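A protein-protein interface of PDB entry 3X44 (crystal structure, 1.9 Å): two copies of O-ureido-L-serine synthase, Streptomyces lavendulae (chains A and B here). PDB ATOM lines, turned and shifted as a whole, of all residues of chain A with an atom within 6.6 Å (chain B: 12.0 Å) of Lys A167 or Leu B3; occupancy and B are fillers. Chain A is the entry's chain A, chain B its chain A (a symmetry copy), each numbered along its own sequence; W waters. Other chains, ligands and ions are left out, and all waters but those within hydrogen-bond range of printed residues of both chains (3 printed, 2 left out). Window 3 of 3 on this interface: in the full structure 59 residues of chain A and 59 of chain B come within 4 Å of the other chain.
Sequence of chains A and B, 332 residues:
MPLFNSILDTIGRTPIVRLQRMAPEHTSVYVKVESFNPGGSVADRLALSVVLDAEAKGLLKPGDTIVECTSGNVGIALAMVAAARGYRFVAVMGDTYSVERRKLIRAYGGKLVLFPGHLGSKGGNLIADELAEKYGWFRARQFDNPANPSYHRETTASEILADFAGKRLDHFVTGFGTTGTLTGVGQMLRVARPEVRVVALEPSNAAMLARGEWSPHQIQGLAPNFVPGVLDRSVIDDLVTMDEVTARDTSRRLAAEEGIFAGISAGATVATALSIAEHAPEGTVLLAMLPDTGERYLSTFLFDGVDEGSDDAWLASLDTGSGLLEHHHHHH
Printed residues of chain B within 4 Å of Ile A16: Leu B3 and Phe B4. Printed residues of chain B within 4 Å of Val A17: Phe B4. Of the printed residues of chain B, Arg A18 touches Phe B4 (3.1 Å) and Asn B5 (3.1 Å). Asp A163 touches two residues of chain B. Phe A164 touches just one residue of chain B: Leu B3. No residue of chain B comes within 4 Å of Ala A165. Lys A167 touches just one residue of chain B: Leu B3. No residue of chain B comes within 4 Å of Leu A169. Printed residues of chain A within 4 Å of Pro B2: Asp A163. Leu B3 touches just these residues of chain A: Ile A16, Asp A163, Phe A164 and Lys A167. Of the printed residues of chain A, Asn B5 touches Arg A18 (3.1 Å). The nearest residue of chain B that does not touch Lys A167 is Pro B2 (6.7 Å). The nearest residue of chain A that does not touch Leu B3 is Tyr A30 (4.1 Å).
NH2 of Arg A193 is in hydrogen-bond range of O of Lys A167 (2.8 Å). The backbone carbonyl oxygen (O) of Phe A164 lies within hydrogen-bond range of the guanidinium group (NH1) of Arg A193, 2.8 Å away.
Of the 15 printed residues of chain A, 6 touch a printed residue of chain B. Printed residues of chain A that touch a printed residue of chain B: Ile A16, Val A17, Arg A18, Asp A163, Phe A164 and Lys A167. Hydrophobic or aromatic side chains of chain A within 4 Å of the printed part of chain B: Ile A16, Val A17 and Phe A164. Among the printed residues, no Asp or Glu carboxylate lies within 4 Å of a Lys or Arg side-chain nitrogen of the other chain.
Water W3 lies within hydrogen-bond range of the backbone carbonyl oxygen of Asp A163 (2.7 Å) and the backbone NH of Leu B3 (3.1 Å). Water W2 lies within hydrogen-bond range of OD2 of Asp A163 (2.7 Å), O of Pro B2 (2.9 Å) and N of Ile A16 (2.9 Å). Water W1 lies within hydrogen-bond range of the backbone carbonyl oxygen (O) of Arg A18 (2.9 Å) and the backbone NH (N) of Ile B7 (3.0 Å).
Among the printed residues, merely in contact across the chains: Val A17 with Phe B4 (3.3 Å), Ile A16 with Leu B3 (3.3 Å), Asp A163 with Leu B3 (3.6 Å), Phe A164 with Leu B3 (3.9 Å) and Lys A167 with Leu B3 (3.96 Å).
No position is printed for both chains. Of the 9 pairs that touch across the chains among the printed residues, none has its exchanged pair printed and touching as well.
O of Arg A18 lies close to O of Asn B5, 3.1 Å away. The side-chain carboxylate (OD1) of Asp A163 sits close to the backbone nitrogen (N) of Pro B2 (3.1 Å). The backbone NH of Arg A18 is in hydrogen-bond range of the backbone carbonyl oxygen of Phe B4 (3.1 Å). N of Phe B4 lies within hydrogen-bond range of O of Ile A16, at 3.0 Å.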
ATOM      1  N   ILE A  16     -28.534 -17.404 -22.627  1.00  0.00           N
ATOM      2  CA  ILE A  16     -29.332 -17.773 -23.781  1.00  0.00           C
ATOM      3  C   ILE A  16     -28.249 -18.027 -24.825  1.00  0.00           C
ATOM      4  O   ILE A  16     -27.396 -17.170 -25.070  1.00  0.00           O
ATOM      5  CB  ILE A  16     -30.260 -16.628 -24.252  1.00  0.00           C
ATOM      6  CG1 ILE A  16     -31.425 -16.464 -23.272  1.00  0.00           C
ATOM      7  CG2 ILE A  16     -30.833 -16.949 -25.641  1.00  0.00           C
ATOM      8  CD1 ILE A  16     -32.352 -15.324 -23.636  1.00  0.00           C
ATOM      9  N   VAL A  17     -28.262 -19.210 -25.417  1.00  0.00           N
ATOM     10  CA  VAL A  17     -27.254 -19.572 -26.401  1.00  0.00           C
ATOM     11  C   VAL A  17     -27.860 -20.057 -27.714  1.00  0.00           C
ATOM     12  O   VAL A  17     -28.956 -20.628 -27.749  1.00  0.00           O
ATOM     13  CB  VAL A  17     -26.309 -20.676 -25.842  1.00  0.00           C
ATOM     14  CG1 VAL A  17     -26.219 -20.562 -24.326  1.00  0.00           C
ATOM     15  CG2 VAL A  17     -26.822 -22.065 -26.226  1.00  0.00           C
ATOM     16  N   ARG A  18     -27.122 -19.844 -28.794  1.00  0.00           N
ATOM     17  CA  ARG A  18     -27.578 -20.248 -30.112  1.00  0.00           C
ATOM     18  C   ARG A  18     -27.256 -21.713 -30.385  1.00  0.00           C
ATOM     19  O   ARG A  18     -26.191 -22.199 -30.005  1.00  0.00           O
ATOM     20  CB  ARG A  18     -26.899 -19.368 -31.165  1.00  0.00           C
ATOM     21  CG  ARG A  18     -27.370 -19.566 -32.590  1.00  0.00           C
ATOM     22  CD  ARG A  18     -26.742 -18.514 -33.491  1.00  0.00           C
ATOM     23  NE  ARG A  18     -27.068 -18.716 -34.900  1.00  0.00           N
ATOM     24  CZ  ARG A  18     -26.578 -19.703 -35.646  1.00  0.00           C
ATOM     25  NH1 ARG A  18     -25.737 -20.584 -35.122  1.00  0.00           N
ATOM     26  NH2 ARG A  18     -26.934 -19.812 -36.920  1.00  0.00           N
ATOM     27  N   TYR A  30     -32.402 -20.130 -30.541  1.00  0.00           N
ATOM     28  CA  TYR A  30     -31.684 -19.842 -29.309  1.00  0.00           C
ATOM     29  C   TYR A  30     -32.404 -20.563 -28.181  1.00  0.00           C
ATOM     30  O   TYR A  30     -33.590 -20.855 -28.295  1.00  0.00           O
ATOM     31  CB  TYR A  30     -31.669 -18.337 -29.051  1.00  0.00           C
ATOM     32  CG  TYR A  30     -30.751 -17.552 -29.968  1.00  0.00           C
ATOM     33  CD1 TYR A  30     -31.222 -17.023 -31.170  1.00  0.00           C
ATOM     34  CD2 TYR A  30     -29.419 -17.311 -29.616  1.00  0.00           C
ATOM     35  CE1 TYR A  30     -30.392 -16.267 -31.996  1.00  0.00           C
ATOM     36  CE2 TYR A  30     -28.583 -16.552 -30.444  1.00  0.00           C
ATOM     37  CZ  TYR A  30     -29.078 -16.035 -31.627  1.00  0.00           C
ATOM     38  OH  TYR A  30     -28.268 -15.271 -32.431  1.00  0.00           O
ATOM     39  N   ILE A 160     -34.612 -11.908 -21.239  1.00  0.00           N
ATOM     40  CA  ILE A 160     -34.919 -12.209 -22.632  1.00  0.00           C
ATOM     41  C   ILE A 160     -34.954 -10.924 -23.461  1.00  0.00           C
ATOM     42  O   ILE A 160     -34.314 -10.835 -24.505  1.00  0.00           O
ATOM     43  CB  ILE A 160     -36.279 -12.947 -22.750  1.00  0.00           C
ATOM     44  CG1 ILE A 160     -36.128 -14.388 -22.244  1.00  0.00           C
ATOM     45  CG2 ILE A 160     -36.772 -12.929 -24.207  1.00  0.00           C
ATOM     46  CD1 ILE A 160     -37.454 -15.148 -22.063  1.00  0.00           C
ATOM     47  N   ALA A 162     -33.673  -7.963 -22.754  1.00  0.00           N
ATOM     48  CA  ALA A 162     -32.374  -7.294 -22.756  1.00  0.00           C
ATOM     49  C   ALA A 162     -31.450  -7.940 -23.781  1.00  0.00           C
ATOM     50  O   ALA A 162     -30.769  -7.251 -24.540  1.00  0.00           O
ATOM     51  CB  ALA A 162     -31.732  -7.366 -21.365  1.00  0.00           C
ATOM     52  N   ASP A 163     -31.435  -9.268 -23.804  1.00  0.00           N
ATOM     53  CA  ASP A 163     -30.584 -10.002 -24.732  1.00  0.00           C
ATOM     54  C   ASP A 163     -30.970  -9.786 -26.192  1.00  0.00           C
ATOM     55  O   ASP A 163     -30.108  -9.759 -27.071  1.00  0.00           O
ATOM     56  CB  ASP A 163     -30.628 -11.497 -24.420  1.00  0.00           C
ATOM     57  CG  ASP A 163     -29.660 -11.895 -23.326  1.00  0.00           C
ATOM     58  OD1 ASP A 163     -28.832 -11.061 -22.914  1.00  0.00           O
ATOM     59  OD2 ASP A 163     -29.728 -13.052 -22.878  1.00  0.00           O
ATOM     60  N   PHE A 164     -32.265  -9.629 -26.451  1.00  0.00           N
ATOM     61  CA  PHE A 164     -32.734  -9.440 -27.816  1.00  0.00           C
ATOM     62  C   PHE A 164     -33.021  -7.997 -28.206  1.00  0.00           C
ATOM     63  O   PHE A 164     -33.502  -7.738 -29.308  1.00  0.00           O
ATOM     64  CB  PHE A 164     -33.977 -10.300 -28.060  1.00  0.00           C
ATOM     65  CG  PHE A 164     -33.657 -11.729 -28.399  1.00  0.00           C
ATOM     66  CD1 PHE A 164     -33.765 -12.726 -27.438  1.00  0.00           C
ATOM     67  CD2 PHE A 164     -33.208 -12.073 -29.673  1.00  0.00           C
ATOM     68  CE1 PHE A 164     -33.431 -14.044 -27.736  1.00  0.00           C
ATOM     69  CE2 PHE A 164     -32.870 -13.389 -29.985  1.00  0.00           C
ATOM     70  CZ  PHE A 164     -32.981 -14.376 -29.014  1.00  0.00           C
ATOM     71  N   ALA A 165     -32.724  -7.060 -27.310  1.00  0.00           N
ATOM     72  CA  ALA A 165     -32.957  -5.646 -27.597  1.00  0.00           C
ATOM     73  C   ALA A 165     -32.164  -5.240 -28.833  1.00  0.00           C
ATOM     74  O   ALA A 165     -30.960  -5.481 -28.918  1.00  0.00           O
ATOM     75  CB  ALA A 165     -32.552  -4.786 -26.405  1.00  0.00           C
ATOM     76  N   GLY A 166     -32.854  -4.637 -29.795  1.00  0.00           N
ATOM     77  CA  GLY A 166     -32.212  -4.206 -31.022  1.00  0.00           C
ATOM     78  C   GLY A 166     -31.955  -5.358 -31.977  1.00  0.00           C
ATOM     79  O   GLY A 166     -31.315  -5.176 -33.016  1.00  0.00           O
ATOM     80  N   LYS A 167     -32.462  -6.540 -31.631  1.00  0.00           N
ATOM     81  CA  LYS A 167     -32.274  -7.735 -32.453  1.00  0.00           C
ATOM     82  C   LYS A 167     -33.581  -8.401 -32.865  1.00  0.00           C
ATOM     83  O   LYS A 167     -34.628  -8.180 -32.261  1.00  0.00           O
ATOM     84  CB  LYS A 167     -31.408  -8.747 -31.708  1.00  0.00           C
ATOM     85  CG  LYS A 167     -29.951  -8.333 -31.589  1.00  0.00           C
ATOM     86  CD  LYS A 167     -29.260  -9.095 -30.480  1.00  0.00           C
ATOM     87  CE  LYS A 167     -28.024  -8.352 -29.994  1.00  0.00           C
ATOM     88  NZ  LYS A 167     -27.128  -7.970 -31.124  1.00  0.00           N
ATOM     89  N   ARG A 168     -33.508  -9.231 -33.897  1.00  0.00           N
ATOM     90  CA  ARG A 168     -34.688  -9.926 -34.397  1.00  0.00           C
ATOM     91  C   ARG A 168     -35.103 -11.125 -33.543  1.00  0.00           C
ATOM     92  O   ARG A 168     -34.278 -11.968 -33.189  1.00  0.00           O
ATOM     93  CB  ARG A 168     -34.449 -10.393 -35.832  1.00  0.00           C
ATOM     94  CG  ARG A 168     -35.538 -11.314 -36.369  1.00  0.00           C
ATOM     95  CD  ARG A 168     -35.586 -11.298 -37.888  1.00  0.00           C
ATOM     96  NE  ARG A 168     -36.682 -12.116 -38.402  1.00  0.00           N
ATOM     97  CZ  ARG A 168     -36.819 -12.460 -39.678  1.00  0.00           C
ATOM     98  NH1 ARG A 168     -35.925 -12.054 -40.574  1.00  0.00           N
ATOM     99  NH2 ARG A 168     -37.841 -13.219 -40.058  1.00  0.00           N
ATOM    100  N   LEU A 169     -36.390 -11.179 -33.213  1.00  0.00           N
ATOM    101  CA  LEU A 169     -36.970 -12.272 -32.439  1.00  0.00           C
ATOM    102  C   LEU A 169     -38.388 -12.459 -32.972  1.00  0.00           C
ATOM    103  O   LEU A 169     -39.197 -11.531 -32.931  1.00  0.00           O
ATOM    104  CB  LEU A 169     -37.006 -11.948 -30.938  1.00  0.00           C
ATOM    105  CG  LEU A 169     -37.616 -13.057 -30.064  1.00  0.00           C
ATOM    106  CD1 LEU A 169     -36.815 -14.342 -30.226  1.00  0.00           C
ATOM    107  CD2 LEU A 169     -37.643 -12.618 -28.600  1.00  0.00           C
ATOM    108  N   ARG A 193     -42.837  -6.334 -27.111  1.00  0.00           N
ATOM    109  CA  ARG A 193     -42.665  -6.887 -28.450  1.00  0.00           C
ATOM    110  C   ARG A 193     -43.874  -7.715 -28.882  1.00  0.00           C
ATOM    111  O   ARG A 193     -43.784  -8.935 -29.050  1.00  0.00           O
ATOM    112  CB  ARG A 193     -41.382  -7.735 -28.512  1.00  0.00           C
ATOM    113  CG  ARG A 193     -40.142  -7.032 -27.932  1.00  0.00           C
ATOM    114  CD  ARG A 193     -38.835  -7.792 -28.218  1.00  0.00           C
ATOM    115  NE  ARG A 193     -38.622  -7.981 -29.653  1.00  0.00           N
ATOM    116  CZ  ARG A 193     -37.433  -8.053 -30.245  1.00  0.00           C
ATOM    117  NH1 ARG A 193     -36.313  -7.954 -29.534  1.00  0.00           N
ATOM    118  NH2 ARG A 193     -37.365  -8.219 -31.560  1.00  0.00           N
ATOM    119  N   LEU A 287     -36.766 -18.568 -29.922  1.00  0.00           N
ATOM    120  CA  LEU A 287     -36.208 -18.779 -28.591  1.00  0.00           C
ATOM    121  C   LEU A 287     -37.004 -19.862 -27.866  1.00  0.00           C
ATOM    122  O   LEU A 287     -38.233 -19.774 -27.762  1.00  0.00           O
ATOM    123  CB  LEU A 287     -36.265 -17.491 -27.773  1.00  0.00           C
ATOM    124  CG  LEU A 287     -35.830 -17.634 -26.312  1.00  0.00           C
ATOM    125  CD1 LEU A 287     -34.322 -17.921 -26.265  1.00  0.00           C
ATOM    126  CD2 LEU A 287     -36.160 -16.360 -25.538  1.00  0.00           C
ATOM    127  N   PRO B   2     -25.836 -10.508 -22.322  1.00  0.00           N
ATOM    128  CA  PRO B   2     -25.884 -10.582 -23.798  1.00  0.00           C
ATOM    129  C   PRO B   2     -25.929 -12.024 -24.291  1.00  0.00           C
ATOM    130  O   PRO B   2     -25.527 -12.950 -23.585  1.00  0.00           O
ATOM    131  CB  PRO B   2     -24.654  -9.879 -24.354  1.00  0.00           C
ATOM    132  CG  PRO B   2     -23.818  -9.579 -23.099  1.00  0.00           C
ATOM    133  CD  PRO B   2     -24.736  -9.633 -21.878  1.00  0.00           C
ATOM    134  N   LEU B   3     -26.413 -12.197 -25.515  1.00  0.00           N
ATOM    135  CA  LEU B   3     -26.531 -13.507 -26.142  1.00  0.00           C
ATOM    136  C   LEU B   3     -25.184 -14.209 -26.307  1.00  0.00           C
ATOM    137  O   LEU B   3     -24.161 -13.564 -26.532  1.00  0.00           O
ATOM    138  CB  LEU B   3     -27.185 -13.362 -27.518  1.00  0.00           C
ATOM    139  CG  LEU B   3     -28.680 -13.049 -27.549  1.00  0.00           C
ATOM    140  CD1 LEU B   3     -29.109 -12.763 -28.986  1.00  0.00           C
ATOM    141  CD2 LEU B   3     -29.452 -14.221 -26.984  1.00  0.00           C
ATOM    142  N   PHE B   4     -25.201 -15.533 -26.198  1.00  0.00           N
ATOM    143  CA  PHE B   4     -23.999 -16.345 -26.365  1.00  0.00           C
ATOM    144  C   PHE B   4     -24.137 -17.120 -27.670  1.00  0.00           C
ATOM    145  O   PHE B   4     -25.232 -17.559 -28.018  1.00  0.00           O
ATOM    146  CB  PHE B   4     -23.850 -17.345 -25.218  1.00  0.00           C
ATOM    147  CG  PHE B   4     -23.532 -16.716 -23.897  1.00  0.00           C
ATOM    148  CD1 PHE B   4     -24.541 -16.453 -22.979  1.00  0.00           C
ATOM    149  CD2 PHE B   4     -22.219 -16.408 -23.556  1.00  0.00           C
ATOM    150  CE1 PHE B   4     -24.251 -15.891 -21.732  1.00  0.00           C
ATOM    151  CE2 PHE B   4     -21.916 -15.847 -22.310  1.00  0.00           C
ATOM    152  CZ  PHE B   4     -22.941 -15.588 -21.397  1.00  0.00           C
ATOM    153  N   ASN B   5     -23.031 -17.280 -28.390  1.00  0.00           N
ATOM    154  CA  ASN B   5     -23.048 -18.016 -29.648  1.00  0.00           C
ATOM    155  C   ASN B   5     -22.993 -19.509 -29.374  1.00  0.00           C
ATOM    156  O   ASN B   5     -23.753 -20.282 -29.951  1.00  0.00           O
ATOM    157  CB  ASN B   5     -21.854 -17.627 -30.520  1.00  0.00           C
ATOM    158  CG  ASN B   5     -21.771 -18.452 -31.792  1.00  0.00           C
ATOM    159  OD1 ASN B   5     -22.791 -18.762 -32.414  1.00  0.00           O
ATOM    160  ND2 ASN B   5     -20.554 -18.818 -32.183  1.00  0.00           N
ATOM    161  N   SER B   6     -22.085 -19.913 -28.492  1.00  0.00           N
ATOM    162  CA  SER B   6     -21.940 -21.322 -28.150  1.00  0.00           C
ATOM    163  C   SER B   6     -22.084 -21.543 -26.657  1.00  0.00           C
ATOM    164  O   SER B   6     -21.817 -20.646 -25.859  1.00  0.00           O
ATOM    165  CB  SER B   6     -20.572 -21.844 -28.606  1.00  0.00           C
ATOM    166  OG  SER B   6     -20.315 -23.143 -28.092  1.00  0.00           O
ATOM    167  N   ILE B   7     -22.501 -22.749 -26.291  1.00  0.00           N
ATOM    168  CA  ILE B   7     -22.666 -23.119 -24.889  1.00  0.00           C
ATOM    169  C   ILE B   7     -21.298 -23.089 -24.200  1.00  0.00           C
ATOM    170  O   ILE B   7     -21.195 -22.865 -22.990  1.00  0.00           O
ATOM    171  CB  ILE B   7     -23.293 -24.536 -24.761  1.00  0.00           C
ATOM    172  CG1 ILE B   7     -23.530 -24.874 -23.285  1.00  0.00           C
ATOM    173  CG2 ILE B   7     -22.384 -25.578 -25.400  1.00  0.00           C
ATOM    174  CD1 ILE B   7     -24.693 -24.111 -22.666  1.00  0.00           C
ATOM    175  N   LEU B   8     -20.240 -23.287 -24.983  1.00  0.00           N
ATOM    176  CA  LEU B   8     -18.887 -23.280 -24.428  1.00  0.00           C
ATOM    177  C   LEU B   8     -18.460 -21.878 -23.994  1.00  0.00           C
ATOM    178  O   LEU B   8     -17.452 -21.717 -23.301  1.00  0.00           O
ATOM    179  CB  LEU B   8     -17.882 -23.827 -25.450  1.00  0.00           C
ATOM    180  CG  LEU B   8     -18.179 -25.168 -26.136  1.00  0.00           C
ATOM    181  CD1 LEU B   8     -16.963 -25.596 -26.963  1.00  0.00           C
ATOM    182  CD2 LEU B   8     -18.528 -26.230 -25.101  1.00  0.00           C
ATOM    183  N   ASP B   9     -19.220 -20.862 -24.402  1.00  0.00           N
ATOM    184  CA  ASP B   9     -18.886 -19.488 -24.037  1.00  0.00           C
ATOM    185  C   ASP B   9     -19.394 -19.149 -22.633  1.00  0.00           C
ATOM    186  O   ASP B   9     -19.199 -18.036 -22.142  1.00  0.00           O
ATOM    187  CB  ASP B   9     -19.469 -18.502 -25.063  1.00  0.00           C
ATOM    188  CG  ASP B   9     -18.893 -18.703 -26.459  1.00  0.00           C
ATOM    189  OD1 ASP B   9     -17.733 -19.153 -26.568  1.00  0.00           O
ATOM    190  OD2 ASP B   9     -19.602 -18.422 -27.449  1.00  0.00           O
ATOM    191  N   THR B  10     -20.041 -20.119 -21.991  1.00  0.00           N
ATOM    192  CA  THR B  10     -20.561 -19.922 -20.641  1.00  0.00           C
ATOM    193  C   THR B  10     -19.661 -20.610 -19.632  1.00  0.00           C
ATOM    194  O   THR B  10     -19.958 -20.639 -18.442  1.00  0.00           O
ATOM    195  CB  THR B  10     -21.983 -20.493 -20.481  1.00  0.00           C
ATOM    196  OG1 THR B  10     -21.933 -21.925 -20.526  1.00  0.00           O
ATOM    197  CG2 THR B  10     -22.895 -19.972 -21.587  1.00  0.00           C
ATOM    198  N   ILE B  11     -18.559 -21.172 -20.116  1.00  0.00           N
ATOM    199  CA  ILE B  11     -17.621 -21.850 -19.237  1.00  0.00           C
ATOM    200  C   ILE B  11     -16.812 -20.840 -18.414  1.00  0.00           C
ATOM    201  O   ILE B  11     -16.346 -19.824 -18.934  1.00  0.00           O
ATOM    202  CB  ILE B  11     -16.662 -22.760 -20.048  1.00  0.00           C
ATOM    203  CG1 ILE B  11     -17.408 -24.024 -20.491  1.00  0.00           C
ATOM    204  CG2 ILE B  11     -15.434 -23.117 -19.210  1.00  0.00           C
ATOM    205  CD1 ILE B  11     -16.636 -24.912 -21.449  1.00  0.00           C
ATOM    206  N   ARG B  13     -16.154 -18.204 -14.995  1.00  0.00           N
ATOM    207  CA  ARG B  13     -16.842 -17.126 -14.306  1.00  0.00           C
ATOM    208  C   ARG B  13     -17.895 -17.653 -13.336  1.00  0.00           C
ATOM    209  O   ARG B  13     -19.060 -17.260 -13.387  1.00  0.00           O
ATOM    210  CB  ARG B  13     -17.485 -16.179 -15.328  1.00  0.00           C
ATOM    211  CG  ARG B  13     -16.467 -15.369 -16.116  1.00  0.00           C
ATOM    212  CD  ARG B  13     -17.122 -14.566 -17.227  1.00  0.00           C
ATOM    213  NE  ARG B  13     -18.152 -15.333 -17.928  1.00  0.00           N
ATOM    214  CZ  ARG B  13     -17.933 -16.083 -19.003  1.00  0.00           C
ATOM    215  NH1 ARG B  13     -16.714 -16.177 -19.518  1.00  0.00           N
ATOM    216  NH2 ARG B  13     -18.939 -16.747 -19.565  1.00  0.00           N
HETATM  217  O   HOH W   1     -24.465 -23.814 -28.247  1.00  0.00           O
HETATM  218  O   HOH W   2     -27.583 -14.632 -22.306  1.00  0.00           O
HETATM  219  O   HOH W   3     -27.465  -9.469 -26.525  1.00  0.00           O
